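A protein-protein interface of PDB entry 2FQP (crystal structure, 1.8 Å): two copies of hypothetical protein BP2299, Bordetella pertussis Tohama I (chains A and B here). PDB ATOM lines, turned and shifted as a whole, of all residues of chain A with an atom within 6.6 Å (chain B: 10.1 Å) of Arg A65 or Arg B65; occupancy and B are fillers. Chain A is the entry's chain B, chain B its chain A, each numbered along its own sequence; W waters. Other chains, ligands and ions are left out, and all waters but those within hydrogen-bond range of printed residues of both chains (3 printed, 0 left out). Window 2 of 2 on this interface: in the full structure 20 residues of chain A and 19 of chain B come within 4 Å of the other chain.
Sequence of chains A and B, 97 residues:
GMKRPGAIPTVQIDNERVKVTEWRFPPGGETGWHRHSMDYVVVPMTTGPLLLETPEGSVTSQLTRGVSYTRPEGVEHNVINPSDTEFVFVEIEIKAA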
ATOM      1  N   GLU A  22     -14.298  13.205 -26.960  1.00  0.00           N
ATOM      2  CA  GLU A  22     -15.110  12.567 -27.969  1.00  0.00           C
ATOM      3  C   GLU A  22     -14.625  11.138 -28.151  1.00  0.00           C
ATOM      4  O   GLU A  22     -13.443  10.917 -28.431  1.00  0.00           O
ATOM      5  CB  GLU A  22     -14.968  13.285 -29.323  1.00  0.00           C
ATOM      6  CG  GLU A  22     -15.803  12.626 -30.383  1.00  0.00           C
ATOM      7  CD  GLU A  22     -15.454  13.014 -31.804  1.00  0.00           C
ATOM      8  OE1 GLU A  22     -14.311  12.753 -32.258  1.00  0.00           O
ATOM      9  OE2 GLU A  22     -16.334  13.589 -32.450  1.00  0.00           O
ATOM     10  N   ARG A  24     -15.140   8.073 -30.679  1.00  0.00           N
ATOM     11  CA  ARG A  24     -15.655   7.673 -31.984  1.00  0.00           C
ATOM     12  C   ARG A  24     -15.332   6.204 -32.167  1.00  0.00           C
ATOM     13  O   ARG A  24     -14.164   5.841 -32.223  1.00  0.00           O
ATOM     14  CB  ARG A  24     -15.013   8.536 -33.055  1.00  0.00           C
ATOM     15  CG  ARG A  24     -15.521   8.360 -34.431  1.00  0.00           C
ATOM     16  CD  ARG A  24     -14.981   9.502 -35.305  1.00  0.00           C
ATOM     17  NE  ARG A  24     -15.555  10.766 -34.883  1.00  0.00           N
ATOM     18  CZ  ARG A  24     -16.696  11.295 -35.349  1.00  0.00           C
ATOM     19  NH1 ARG A  24     -17.418  10.691 -36.266  1.00  0.00           N
ATOM     20  NH2 ARG A  24     -17.143  12.449 -34.869  1.00  0.00           N
ATOM     21  N   VAL A  43     -22.913  12.553 -23.213  1.00  0.00           N
ATOM     22  CA  VAL A  43     -23.830  13.024 -24.229  1.00  0.00           C
ATOM     23  C   VAL A  43     -23.730  12.194 -25.508  1.00  0.00           C
ATOM     24  O   VAL A  43     -22.770  12.342 -26.306  1.00  0.00           O
ATOM     25  CB  VAL A  43     -23.618  14.537 -24.578  1.00  0.00           C
ATOM     26  CG1 VAL A  43     -24.678  15.004 -25.556  1.00  0.00           C
ATOM     27  CG2 VAL A  43     -23.666  15.402 -23.273  1.00  0.00           C
ATOM     28  N   PRO A  44     -24.728  11.314 -25.731  1.00  0.00           N
ATOM     29  CA  PRO A  44     -24.700  10.510 -26.927  1.00  0.00           C
ATOM     30  C   PRO A  44     -24.922  11.321 -28.168  1.00  0.00           C
ATOM     31  O   PRO A  44     -25.786  12.196 -28.170  1.00  0.00           O
ATOM     32  CB  PRO A  44     -25.844   9.520 -26.722  1.00  0.00           C
ATOM     33  CG  PRO A  44     -26.083   9.504 -25.239  1.00  0.00           C
ATOM     34  CD  PRO A  44     -25.840  10.929 -24.857  1.00  0.00           C
ATOM     35  N   MET A  45     -24.110  11.044 -29.194  1.00  0.00           N
ATOM     36  CA  MET A  45     -24.242  11.772 -30.463  1.00  0.00           C
ATOM     37  C   MET A  45     -24.888  10.850 -31.497  1.00  0.00           C
ATOM     38  O   MET A  45     -25.181  11.271 -32.618  1.00  0.00           O
ATOM     39  CB  MET A  45     -22.899  12.236 -30.991  1.00  0.00           C
ATOM     40  CG  MET A  45     -22.139  13.140 -30.085  1.00  0.00           C
ATOM     41  SD  MET A  45     -23.134  14.722 -29.513  1.00  0.00           S
ATOM     42  CE  MET A  45     -23.624  15.292 -31.327  1.00  0.00           C
ATOM     43  N   THR A  46     -25.142   9.612 -31.098  1.00  0.00           N
ATOM     44  CA  THR A  46     -25.691   8.559 -31.952  1.00  0.00           C
ATOM     45  C   THR A  46     -26.724   7.813 -31.139  1.00  0.00           C
ATOM     46  O   THR A  46     -26.536   7.617 -29.951  1.00  0.00           O
ATOM     47  CB  THR A  46     -24.583   7.502 -32.285  1.00  0.00           C
ATOM     48  OG1 THR A  46     -23.494   8.131 -32.934  1.00  0.00           O
ATOM     49  CG2 THR A  46     -25.117   6.428 -33.177  1.00  0.00           C
ATOM     50  N   THR A  47     -27.814   7.392 -31.752  1.00  0.00           N
ATOM     51  CA  THR A  47     -28.774   6.525 -31.066  1.00  0.00           C
ATOM     52  C   THR A  47     -28.400   5.105 -31.395  1.00  0.00           C
ATOM     53  O   THR A  47     -28.265   4.754 -32.550  1.00  0.00           O
ATOM     54  CB  THR A  47     -30.205   6.759 -31.547  1.00  0.00           C
ATOM     55  OG1 THR A  47     -30.645   8.072 -31.171  1.00  0.00           O
ATOM     56  CG2 THR A  47     -31.156   5.701 -30.972  1.00  0.00           C
ATOM     57  N   GLY A  48     -28.302   4.275 -30.385  1.00  0.00           N
ATOM     58  CA  GLY A  48     -28.014   2.906 -30.622  1.00  0.00           C
ATOM     59  C   GLY A  48     -27.530   2.236 -29.375  1.00  0.00           C
ATOM     60  O   GLY A  48     -27.332   2.853 -28.340  1.00  0.00           O
ATOM     61  N   LEU A  63     -28.466   3.840 -25.834  1.00  0.00           N
ATOM     62  CA  LEU A  63     -28.215   5.299 -25.810  1.00  0.00           C
ATOM     63  C   LEU A  63     -29.118   5.994 -26.808  1.00  0.00           C
ATOM     64  O   LEU A  63     -29.443   5.438 -27.854  1.00  0.00           O
ATOM     65  CB  LEU A  63     -26.743   5.546 -26.129  1.00  0.00           C
ATOM     66  CG  LEU A  63     -25.848   5.525 -24.880  1.00  0.00           C
ATOM     67  CD1 LEU A  63     -25.812   4.134 -24.315  1.00  0.00           C
ATOM     68  CD2 LEU A  63     -24.422   5.983 -25.204  1.00  0.00           C
ATOM     69  N   THR A  64     -29.527   7.223 -26.493  1.00  0.00           N
ATOM     70  CA  THR A  64     -30.394   7.973 -27.378  1.00  0.00           C
ATOM     71  C   THR A  64     -29.691   9.312 -27.627  1.00  0.00           C
ATOM     72  O   THR A  64     -29.240   9.970 -26.678  1.00  0.00           O
ATOM     73  CB  THR A  64     -31.812   8.136 -26.744  1.00  0.00           C
ATOM     74  OG1 THR A  64     -32.439   6.832 -26.600  1.00  0.00           O
ATOM     75  CG2 THR A  64     -32.667   8.977 -27.602  1.00  0.00           C
ATOM     76  N   ARG A  65     -29.541   9.661 -28.895  1.00  0.00           N
ATOM     77  CA  ARG A  65     -28.894  10.891 -29.280  1.00  0.00           C
ATOM     78  C   ARG A  65     -29.497  12.049 -28.536  1.00  0.00           C
ATOM     79  O   ARG A  65     -30.736  12.221 -28.496  1.00  0.00           O
ATOM     80  CB  ARG A  65     -29.045  11.159 -30.761  1.00  0.00           C
ATOM     81  CG  ARG A  65     -28.204  12.294 -31.230  1.00  0.00           C
ATOM     82  CD  ARG A  65     -28.143  12.327 -32.754  1.00  0.00           C
ATOM     83  NE  ARG A  65     -27.129  13.294 -33.193  1.00  0.00           N
ATOM     84  CZ  ARG A  65     -27.361  14.592 -33.367  1.00  0.00           C
ATOM     85  NH1 ARG A  65     -28.585  15.087 -33.221  1.00  0.00           N
ATOM     86  NH2 ARG A  65     -26.374  15.380 -33.759  1.00  0.00           N
ATOM     87  N   GLY A  66     -28.616  12.833 -27.931  1.00  0.00           N
ATOM     88  CA  GLY A  66     -29.032  14.029 -27.271  1.00  0.00           C
ATOM     89  C   GLY A  66     -29.583  13.864 -25.859  1.00  0.00           C
ATOM     90  O   GLY A  66     -29.967  14.862 -25.256  1.00  0.00           O
ATOM     91  N   VAL A  67     -29.627  12.637 -25.345  1.00  0.00           N
ATOM     92  CA  VAL A  67     -30.159  12.373 -23.996  1.00  0.00           C
ATOM     93  C   VAL A  67     -29.014  12.024 -23.089  1.00  0.00           C
ATOM     94  O   VAL A  67     -28.510  10.900 -23.063  1.00  0.00           O
ATOM     95  CB  VAL A  67     -31.208  11.308 -23.960  1.00  0.00           C
ATOM     96  CG1 VAL A  67     -31.771  11.148 -22.526  1.00  0.00           C
ATOM     97  CG2 VAL A  67     -32.369  11.694 -24.933  1.00  0.00           C
ATOM     98  N   SER A  68     -28.631  13.007 -22.297  1.00  0.00           N
ATOM     99  CA  SER A  68     -27.475  12.875 -21.467  1.00  0.00           C
ATOM    100  C   SER A  68     -27.785  12.108 -20.183  1.00  0.00           C
ATOM    101  O   SER A  68     -28.930  12.003 -19.760  1.00  0.00           O
ATOM    102  CB  SER A  68     -26.959  14.258 -21.092  1.00  0.00           C
ATOM    103  OG  SER A  68     -27.735  14.833 -20.058  1.00  0.00           O
ATOM    104  N   GLN B  12     -31.999  18.043 -17.996  1.00  0.00           N
ATOM    105  CA  GLN B  12     -31.756  16.589 -18.042  1.00  0.00           C
ATOM    106  C   GLN B  12     -31.132  15.982 -16.781  1.00  0.00           C
ATOM    107  O   GLN B  12     -31.440  14.832 -16.437  1.00  0.00           O
ATOM    108  CB  GLN B  12     -30.926  16.250 -19.291  1.00  0.00           C
ATOM    109  CG  GLN B  12     -31.667  16.519 -20.594  1.00  0.00           C
ATOM    110  CD  GLN B  12     -30.865  16.091 -21.816  1.00  0.00           C
ATOM    111  OE1 GLN B  12     -29.703  15.781 -21.680  1.00  0.00           O
ATOM    112  NE2 GLN B  12     -31.510  15.996 -22.990  1.00  0.00           N
ATOM    113  N   GLU B  22     -30.884  20.837 -21.994  1.00  0.00           N
ATOM    114  CA  GLU B  22     -31.028  20.836 -23.444  1.00  0.00           C
ATOM    115  C   GLU B  22     -31.749  22.127 -23.786  1.00  0.00           C
ATOM    116  O   GLU B  22     -32.824  22.411 -23.219  1.00  0.00           O
ATOM    117  CB  GLU B  22     -31.878  19.662 -23.921  1.00  0.00           C
ATOM    118  CG  GLU B  22     -32.290  19.725 -25.373  1.00  0.00           C
ATOM    119  CD  GLU B  22     -33.393  18.771 -25.691  1.00  0.00           C
ATOM    120  OE1 GLU B  22     -34.514  18.990 -25.152  1.00  0.00           O
ATOM    121  OE2 GLU B  22     -33.124  17.773 -26.414  1.00  0.00           O
ATOM    122  N   ARG B  24     -33.546  24.005 -26.927  1.00  0.00           N
ATOM    123  CA  ARG B  24     -34.078  23.797 -28.273  1.00  0.00           C
ATOM    124  C   ARG B  24     -34.613  25.104 -28.848  1.00  0.00           C
ATOM    125  O   ARG B  24     -35.558  25.701 -28.317  1.00  0.00           O
ATOM    126  CB  ARG B  24     -35.159  22.679 -28.307  1.00  0.00           C
ATOM    127  CG  ARG B  24     -34.649  21.288 -27.978  1.00  0.00           C
ATOM    128  CD  ARG B  24     -35.798  20.237 -27.879  1.00  0.00           C
ATOM    129  NE  ARG B  24     -36.378  19.993 -29.188  1.00  0.00           N
ATOM    130  CZ  ARG B  24     -37.146  18.941 -29.496  1.00  0.00           C
ATOM    131  NH1 ARG B  24     -37.433  18.005 -28.592  1.00  0.00           N
ATOM    132  NH2 ARG B  24     -37.627  18.810 -30.739  1.00  0.00           N
ATOM    133  N   VAL B  42     -20.672  23.634 -23.814  1.00  0.00           N
ATOM    134  CA  VAL B  42     -21.705  23.542 -24.808  1.00  0.00           C
ATOM    135  C   VAL B  42     -21.368  22.351 -25.690  1.00  0.00           C
ATOM    136  O   VAL B  42     -20.269  22.302 -26.256  1.00  0.00           O
ATOM    137  CB  VAL B  42     -21.777  24.855 -25.652  1.00  0.00           C
ATOM    138  CG1 VAL B  42     -22.748  24.722 -26.823  1.00  0.00           C
ATOM    139  CG2 VAL B  42     -22.120  26.053 -24.763  1.00  0.00           C
ATOM    140  N   VAL B  43     -22.284  21.384 -25.764  1.00  0.00           N
ATOM    141  CA  VAL B  43     -22.189  20.317 -26.751  1.00  0.00           C
ATOM    142  C   VAL B  43     -23.272  20.519 -27.813  1.00  0.00           C
ATOM    143  O   VAL B  43     -24.432  20.239 -27.565  1.00  0.00           O
ATOM    144  CB  VAL B  43     -22.394  18.911 -26.113  1.00  0.00           C
ATOM    145  CG1 VAL B  43     -22.182  17.848 -27.171  1.00  0.00           C
ATOM    146  CG2 VAL B  43     -21.432  18.665 -24.914  1.00  0.00           C
ATOM    147  N   PRO B  44     -22.898  21.043 -28.991  1.00  0.00           N
ATOM    148  CA  PRO B  44     -23.913  21.211 -30.011  1.00  0.00           C
ATOM    149  C   PRO B  44     -24.486  19.890 -30.510  1.00  0.00           C
ATOM    150  O   PRO B  44     -23.742  18.920 -30.682  1.00  0.00           O
ATOM    151  CB  PRO B  44     -23.154  21.930 -31.140  1.00  0.00           C
ATOM    152  CG  PRO B  44     -21.987  22.524 -30.490  1.00  0.00           C
ATOM    153  CD  PRO B  44     -21.591  21.518 -29.464  1.00  0.00           C
ATOM    154  N   MET B  45     -25.788  19.866 -30.740  1.00  0.00           N
ATOM    155  CA  MET B  45     -26.481  18.687 -31.279  1.00  0.00           C
ATOM    156  C   MET B  45     -26.862  18.901 -32.742  1.00  0.00           C
ATOM    157  O   MET B  45     -27.369  18.000 -33.393  1.00  0.00           O
ATOM    158  CB  MET B  45     -27.718  18.373 -30.447  1.00  0.00           C
ATOM    159  CG  MET B  45     -27.515  18.055 -28.999  1.00  0.00           C
ATOM    160  SD  MET B  45     -26.172  16.658 -28.648  1.00  0.00           S
ATOM    161  CE  MET B  45     -26.980  15.383 -29.745  1.00  0.00           C
ATOM    162  N   THR B  46     -26.629  20.116 -33.232  1.00  0.00           N
ATOM    163  CA  THR B  46     -26.968  20.578 -34.551  1.00  0.00           C
ATOM    164  C   THR B  46     -25.739  21.263 -35.099  1.00  0.00           C
ATOM    165  O   THR B  46     -25.027  21.953 -34.381  1.00  0.00           O
ATOM    166  CB  THR B  46     -28.074  21.633 -34.503  1.00  0.00           C
ATOM    167  OG1 THR B  46     -29.198  21.132 -33.764  1.00  0.00           O
ATOM    168  CG2 THR B  46     -28.470  22.042 -35.901  1.00  0.00           C
ATOM    169  N   THR B  47     -25.467  21.067 -36.377  1.00  0.00           N
ATOM    170  CA  THR B  47     -24.406  21.850 -37.029  1.00  0.00           C
ATOM    171  C   THR B  47     -25.065  23.054 -37.657  1.00  0.00           C
ATOM    172  O   THR B  47     -26.030  22.915 -38.449  1.00  0.00           O
ATOM    173  CB  THR B  47     -23.697  21.018 -38.078  1.00  0.00           C
ATOM    174  OG1 THR B  47     -23.049  19.922 -37.419  1.00  0.00           O
ATOM    175  CG2 THR B  47     -22.676  21.855 -38.880  1.00  0.00           C
ATOM    176  N   GLY B  48     -24.585  24.233 -37.321  1.00  0.00           N
ATOM    177  CA  GLY B  48     -25.191  25.445 -37.857  1.00  0.00           C
ATOM    178  C   GLY B  48     -24.715  26.688 -37.163  1.00  0.00           C
ATOM    179  O   GLY B  48     -24.050  26.583 -36.124  1.00  0.00           O
ATOM    180  N   PRO B  49     -25.056  27.863 -37.721  1.00  0.00           N
ATOM    181  CA  PRO B  49     -24.671  29.147 -37.120  1.00  0.00           C
ATOM    182  C   PRO B  49     -25.552  29.498 -35.901  1.00  0.00           C
ATOM    183  O   PRO B  49     -26.746  29.135 -35.841  1.00  0.00           O
ATOM    184  CB  PRO B  49     -24.911  30.142 -38.271  1.00  0.00           C
ATOM    185  CG  PRO B  49     -26.069  29.568 -39.006  1.00  0.00           C
ATOM    186  CD  PRO B  49     -25.812  28.051 -38.970  1.00  0.00           C
ATOM    187  N   GLN B  62     -20.007  29.577 -35.827  1.00  0.00           N
ATOM    188  CA  GLN B  62     -20.337  28.347 -36.532  1.00  0.00           C
ATOM    189  C   GLN B  62     -20.152  27.161 -35.612  1.00  0.00           C
ATOM    190  O   GLN B  62     -19.051  26.907 -35.161  1.00  0.00           O
ATOM    191  CB  GLN B  62     -19.425  28.138 -37.736  1.00  0.00           C
ATOM    192  CG  GLN B  62     -19.591  29.133 -38.799  1.00  0.00           C
ATOM    193  CD  GLN B  62     -20.932  29.075 -39.471  1.00  0.00           C
ATOM    194  OE1 GLN B  62     -21.578  28.013 -39.531  1.00  0.00           O
ATOM    195  NE2 GLN B  62     -21.379  30.225 -39.981  1.00  0.00           N
ATOM    196  N   LEU B  63     -21.240  26.488 -35.284  1.00  0.00           N
ATOM    197  CA  LEU B  63     -21.162  25.346 -34.406  1.00  0.00           C
ATOM    198  C   LEU B  63     -21.193  24.033 -35.211  1.00  0.00           C
ATOM    199  O   LEU B  63     -21.844  23.946 -36.256  1.00  0.00           O
ATOM    200  CB  LEU B  63     -22.310  25.387 -33.413  1.00  0.00           C
ATOM    201  CG  LEU B  63     -22.079  26.192 -32.145  1.00  0.00           C
ATOM    202  CD1 LEU B  63     -21.802  27.653 -32.472  1.00  0.00           C
ATOM    203  CD2 LEU B  63     -23.268  26.052 -31.212  1.00  0.00           C
ATOM    204  N   THR B  64     -20.520  23.013 -34.696  1.00  0.00           N
ATOM    205  CA  THR B  64     -20.524  21.693 -35.317  1.00  0.00           C
ATOM    206  C   THR B  64     -21.083  20.711 -34.321  1.00  0.00           C
ATOM    207  O   THR B  64     -20.627  20.667 -33.159  1.00  0.00           O
ATOM    208  CB  THR B  64     -19.115  21.270 -35.699  1.00  0.00           C
ATOM    209  OG1 THR B  64     -18.604  22.235 -36.607  1.00  0.00           O
ATOM    210  CG2 THR B  64     -19.092  19.927 -36.361  1.00  0.00           C
ATOM    211  N   ARG B  65     -22.047  19.895 -34.768  1.00  0.00           N
ATOM    212  CA  ARG B  65     -22.586  18.880 -33.893  1.00  0.00           C
ATOM    213  C   ARG B  65     -21.445  18.045 -33.293  1.00  0.00           C
ATOM    214  O   ARG B  65     -20.533  17.592 -34.001  1.00  0.00           O
ATOM    215  CB  ARG B  65     -23.643  17.985 -34.585  1.00  0.00           C
ATOM    216  CG  ARG B  65     -23.121  17.112 -35.653  1.00  0.00           C
ATOM    217  CD  ARG B  65     -24.266  16.434 -36.427  1.00  0.00           C
ATOM    218  NE  ARG B  65     -23.736  15.487 -37.411  1.00  0.00           N
ATOM    219  CZ  ARG B  65     -24.435  14.499 -37.966  1.00  0.00           C
ATOM    220  NH1 ARG B  65     -25.723  14.315 -37.650  1.00  0.00           N
ATOM    221  NH2 ARG B  65     -23.848  13.683 -38.846  1.00  0.00           N
ATOM    222  N   GLY B  66     -21.497  17.885 -31.976  1.00  0.00           N
ATOM    223  CA  GLY B  66     -20.568  17.041 -31.255  1.00  0.00           C
ATOM    224  C   GLY B  66     -19.214  17.634 -30.979  1.00  0.00           C
ATOM    225  O   GLY B  66     -18.365  16.928 -30.485  1.00  0.00           O
ATOM    226  N   VAL B  67     -18.997  18.891 -31.364  1.00  0.00           N
ATOM    227  CA  VAL B  67     -17.731  19.587 -31.145  1.00  0.00           C
ATOM    228  C   VAL B  67     -17.967  20.570 -30.014  1.00  0.00           C
ATOM    229  O   VAL B  67     -18.547  21.656 -30.197  1.00  0.00           O
ATOM    230  CB  VAL B  67     -17.223  20.320 -32.399  1.00  0.00           C
ATOM    231  CG1 VAL B  67     -15.929  21.051 -32.096  1.00  0.00           C
ATOM    232  CG2 VAL B  67     -17.051  19.342 -33.526  1.00  0.00           C
ATOM    233  N   SER B  68     -17.531  20.172 -28.829  1.00  0.00           N
ATOM    234  CA  SER B  68     -17.807  20.935 -27.629  1.00  0.00           C
ATOM    235  C   SER B  68     -16.862  22.118 -27.462  1.00  0.00           C
ATOM    236  O   SER B  68     -15.793  22.207 -28.064  1.00  0.00           O
ATOM    237  CB  SER B  68     -17.725  20.046 -26.389  1.00  0.00           C
ATOM    238  OG  SER B  68     -16.389  19.729 -26.076  1.00  0.00           O
ATOM    239  N   TYR B  69     -17.303  23.054 -26.646  1.00  0.00           N
ATOM    240  CA  TYR B  69     -16.453  24.141 -26.231  1.00  0.00           C
ATOM    241  C   TYR B  69     -16.885  24.603 -24.865  1.00  0.00           C
ATOM    242  O   TYR B  69     -17.976  24.274 -24.413  1.00  0.00           O
ATOM    243  CB  TYR B  69     -16.509  25.275 -27.233  1.00  0.00           C
ATOM    244  CG  TYR B  69     -17.845  25.897 -27.468  1.00  0.00           C
ATOM    245  CD1 TYR B  69     -18.662  25.429 -28.483  1.00  0.00           C
ATOM    246  CD2 TYR B  69     -18.232  27.026 -26.777  1.00  0.00           C
ATOM    247  CE1 TYR B  69     -19.871  26.015 -28.741  1.00  0.00           C
ATOM    248  CE2 TYR B  69     -19.410  27.654 -27.012  1.00  0.00           C
ATOM    249  CZ  TYR B  69     -20.244  27.149 -28.025  1.00  0.00           C
ATOM    250  OH  TYR B  69     -21.435  27.759 -28.299  1.00  0.00           O
ATOM    251  N   GLU B  86     -34.796  24.041 -36.557  1.00  0.00           N
ATOM    252  CA  GLU B  86     -34.556  23.991 -35.116  1.00  0.00           C
ATOM    253  C   GLU B  86     -33.090  23.781 -34.883  1.00  0.00           C
ATOM    254  O   GLU B  86     -32.463  23.020 -35.626  1.00  0.00           O
ATOM    255  CB  GLU B  86     -35.340  22.837 -34.500  1.00  0.00           C
ATOM    256  CG  GLU B  86     -35.219  22.716 -32.992  1.00  0.00           C
ATOM    257  CD  GLU B  86     -36.191  21.718 -32.407  1.00  0.00           C
ATOM    258  OE1 GLU B  86     -36.455  20.708 -33.078  1.00  0.00           O
ATOM    259  OE2 GLU B  86     -36.702  21.953 -31.284  1.00  0.00           O
ATOM    260  N   PHE B  87     -32.557  24.453 -33.868  1.00  0.00           N
ATOM    261  CA  PHE B  87     -31.168  24.298 -33.441  1.00  0.00           C
ATOM    262  C   PHE B  87     -31.149  23.802 -32.012  1.00  0.00           C
ATOM    263  O   PHE B  87     -31.887  24.305 -31.165  1.00  0.00           O
ATOM    264  CB  PHE B  87     -30.374  25.620 -33.512  1.00  0.00           C
ATOM    265  CG  PHE B  87     -28.918  25.410 -33.373  1.00  0.00           C
ATOM    266  CD1 PHE B  87     -28.337  25.200 -32.124  1.00  0.00           C
ATOM    267  CD2 PHE B  87     -28.102  25.348 -34.520  1.00  0.00           C
ATOM    268  CE1 PHE B  87     -26.978  24.916 -31.986  1.00  0.00           C
ATOM    269  CE2 PHE B  87     -26.749  25.112 -34.401  1.00  0.00           C
ATOM    270  CZ  PHE B  87     -26.171  24.900 -33.125  1.00  0.00           C
ATOM    271  N   VAL B  88     -30.319  22.795 -31.735  1.00  0.00           N
ATOM    272  CA  VAL B  88     -30.296  22.192 -30.402  1.00  0.00           C
ATOM    273  C   VAL B  88     -28.858  22.096 -29.884  1.00  0.00           C
ATOM    274  O   VAL B  88     -27.951  21.790 -30.635  1.00  0.00           O
ATOM    275  CB  VAL B  88     -30.946  20.792 -30.437  1.00  0.00           C
ATOM    276  CG1 VAL B  88     -30.955  20.159 -29.026  1.00  0.00           C
ATOM    277  CG2 VAL B  88     -32.353  20.861 -31.033  1.00  0.00           C
ATOM    278  N   PHE B  89     -28.666  22.446 -28.611  1.00  0.00           N
ATOM    279  CA  PHE B  89     -27.440  22.155 -27.891  1.00  0.00           C
ATOM    280  C   PHE B  89     -27.710  21.751 -26.456  1.00  0.00           C
ATOM    281  O   PHE B  89     -28.773  22.039 -25.898  1.00  0.00           O
ATOM    282  CB  PHE B  89     -26.360  23.273 -27.979  1.00  0.00           C
ATOM    283  CG  PHE B  89     -26.725  24.603 -27.333  1.00  0.00           C
ATOM    284  CD1 PHE B  89     -26.620  24.796 -25.931  1.00  0.00           C
ATOM    285  CD2 PHE B  89     -27.017  25.715 -28.125  1.00  0.00           C
ATOM    286  CE1 PHE B  89     -26.911  26.059 -25.369  1.00  0.00           C
ATOM    287  CE2 PHE B  89     -27.276  26.950 -27.567  1.00  0.00           C
ATOM    288  CZ  PHE B  89     -27.243  27.127 -26.199  1.00  0.00           C
ATOM    289  N   VAL B  90     -26.742  21.024 -25.904  1.00  0.00           N
ATOM    290  CA  VAL B  90     -26.750  20.610 -24.532  1.00  0.00           C
ATOM    291  C   VAL B  90     -25.710  21.455 -23.784  1.00  0.00           C
ATOM    292  O   VAL B  90     -24.550  21.531 -24.194  1.00  0.00           O
ATOM    293  CB  VAL B  90     -26.489  19.087 -24.376  1.00  0.00           C
ATOM    294  CG1 VAL B  90     -26.296  18.708 -22.897  1.00  0.00           C
ATOM    295  CG2 VAL B  90     -27.666  18.312 -24.971  1.00  0.00           C
HETATM  296  O   HOH W   1     -30.599  16.947 -27.045  1.00  0.00           O
HETATM  297  O   HOH W   2     -30.448  17.346 -32.345  1.00  0.00           O
HETATM  298  O   HOH W   3     -18.677  14.202 -31.343  1.00  0.00           O
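Met B45 touches Val A43.
CE of Met B45 touches O of Pro A44 (3.8 Å).
Pro B44 touches Met A45.
Met A45 touches Gly B66 (CE to N, 3.4 Å).
NH2 of Arg A65 touches CD of Arg B65, at 3.6 Å.
Gly A66 touches Met B45.
NE2 of Gln B12 touches CA of Val A67, at 3.995 Å.
O of Pro B44 is in hydrogen-bond range of N of Gly B66.
The backbone carbonyl oxygen of Val B88 sits at hydrogen-bond distance from the backbone NH of Met B45 (2.9 Å).
OG1 of Thr B47 sits at hydrogen-bond distance from N of Arg B65 (2.8 Å).
The backbone carbonyl oxygen (O) of Pro A44 is in hydrogen-bond range of the backbone NH (N) of Gly A66, at 2.9 Å.
The backbone carbonyl oxygen of Met A45 lies within hydrogen-bond range of the guanidinium group of Arg A65 (2.9 Å).
The side-chain hydroxyl of Thr A47 lies within hydrogen-bond range of the backbone NH of Arg A65, 3.0 Å away.
Hydrophobic or aromatic side chains of chain B within 4 Å of the printed part of chain A: Met B45.
Of the 14 printed residues of chain A, 7 touch a printed residue of chain B.
Among the printed residues, 11 pairs touch across the chains.
Arg A65 touches two residues of chain B.
Met A45 touches just these residues of chain B: Pro B44 (3.7 Å), Met B45 (3.7 Å) and Gly B66 (3.4 Å).
Gly A66 touches just these residues of chain B: Gln B12 and Met B45.
Of the printed residues of chain B, Val A43 touches Met B45 (3.8 Å).
Printed residues of chain A within 4 Å of Pro B44: Met A45 (3.7 Å).
Printed residues of chain B within 4 Å of Val A67: Gln B12.
Printed residues of chain A within 4 Å of Gln B12: Gly A66 (3.0 Å), Val A67 (3.995 Å) and Ser A68 (2.7 Å).
Of the printed residues of chain A, Met B45 touches Val A43, Pro A44, Met A45, Arg A65 and Gly A66.
Glu B22 touches none of the printed residues of chain A.
Gly B48 touches none of the printed residues of chain A.
The nearest printed residue of chain B that does not touch Ser A68 is Val B90 (4.8 Å).
Water W3 bridges the side-chain carboxylate (OE2) of Glu A22 (2.7 Å) and the backbone carbonyl oxygen (O) of Gly B66 (2.9 Å).
Water W1 bridges OE2 of Glu B22 (2.7 Å) and O of Gly A66 (2.8 Å).
Water W2 lies within hydrogen-bond range of the guanidinium group (NH1) of Arg A65 (3.1 Å) and the backbone carbonyl oxygen (O) of Met B45 (3.3 Å).
The side-chain amide nitrogen (NE2) of Gln B12 is in hydrogen-bond range of the backbone carbonyl oxygen (O) of Gly A66 (3.0 Å).
The side-chain amide oxygen (OE1) of Gln B12 lies within hydrogen-bond range of the side-chain hydroxyl (OG) of Ser A68.
The backbone carbonyl oxygen (O) of Met B45 is in hydrogen-bond range of the guanidinium group (NH2) of Arg A65, 2.8 Å away.
SD of Met B45 lies close to SD of Met A45 (3.7 Å).
Met B45 touches its own counterpart, Met A45.
Met A45 touches Gly B66, and with the chains exchanged Gly A66 touches Met B45.
Arg A65 touches Met B45, but with the chains exchanged Met A45 does not touch Arg B65 (4.02 Å).
Arg A65 touches its own counterpart, Arg B65.
14 positions are printed for both chains.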
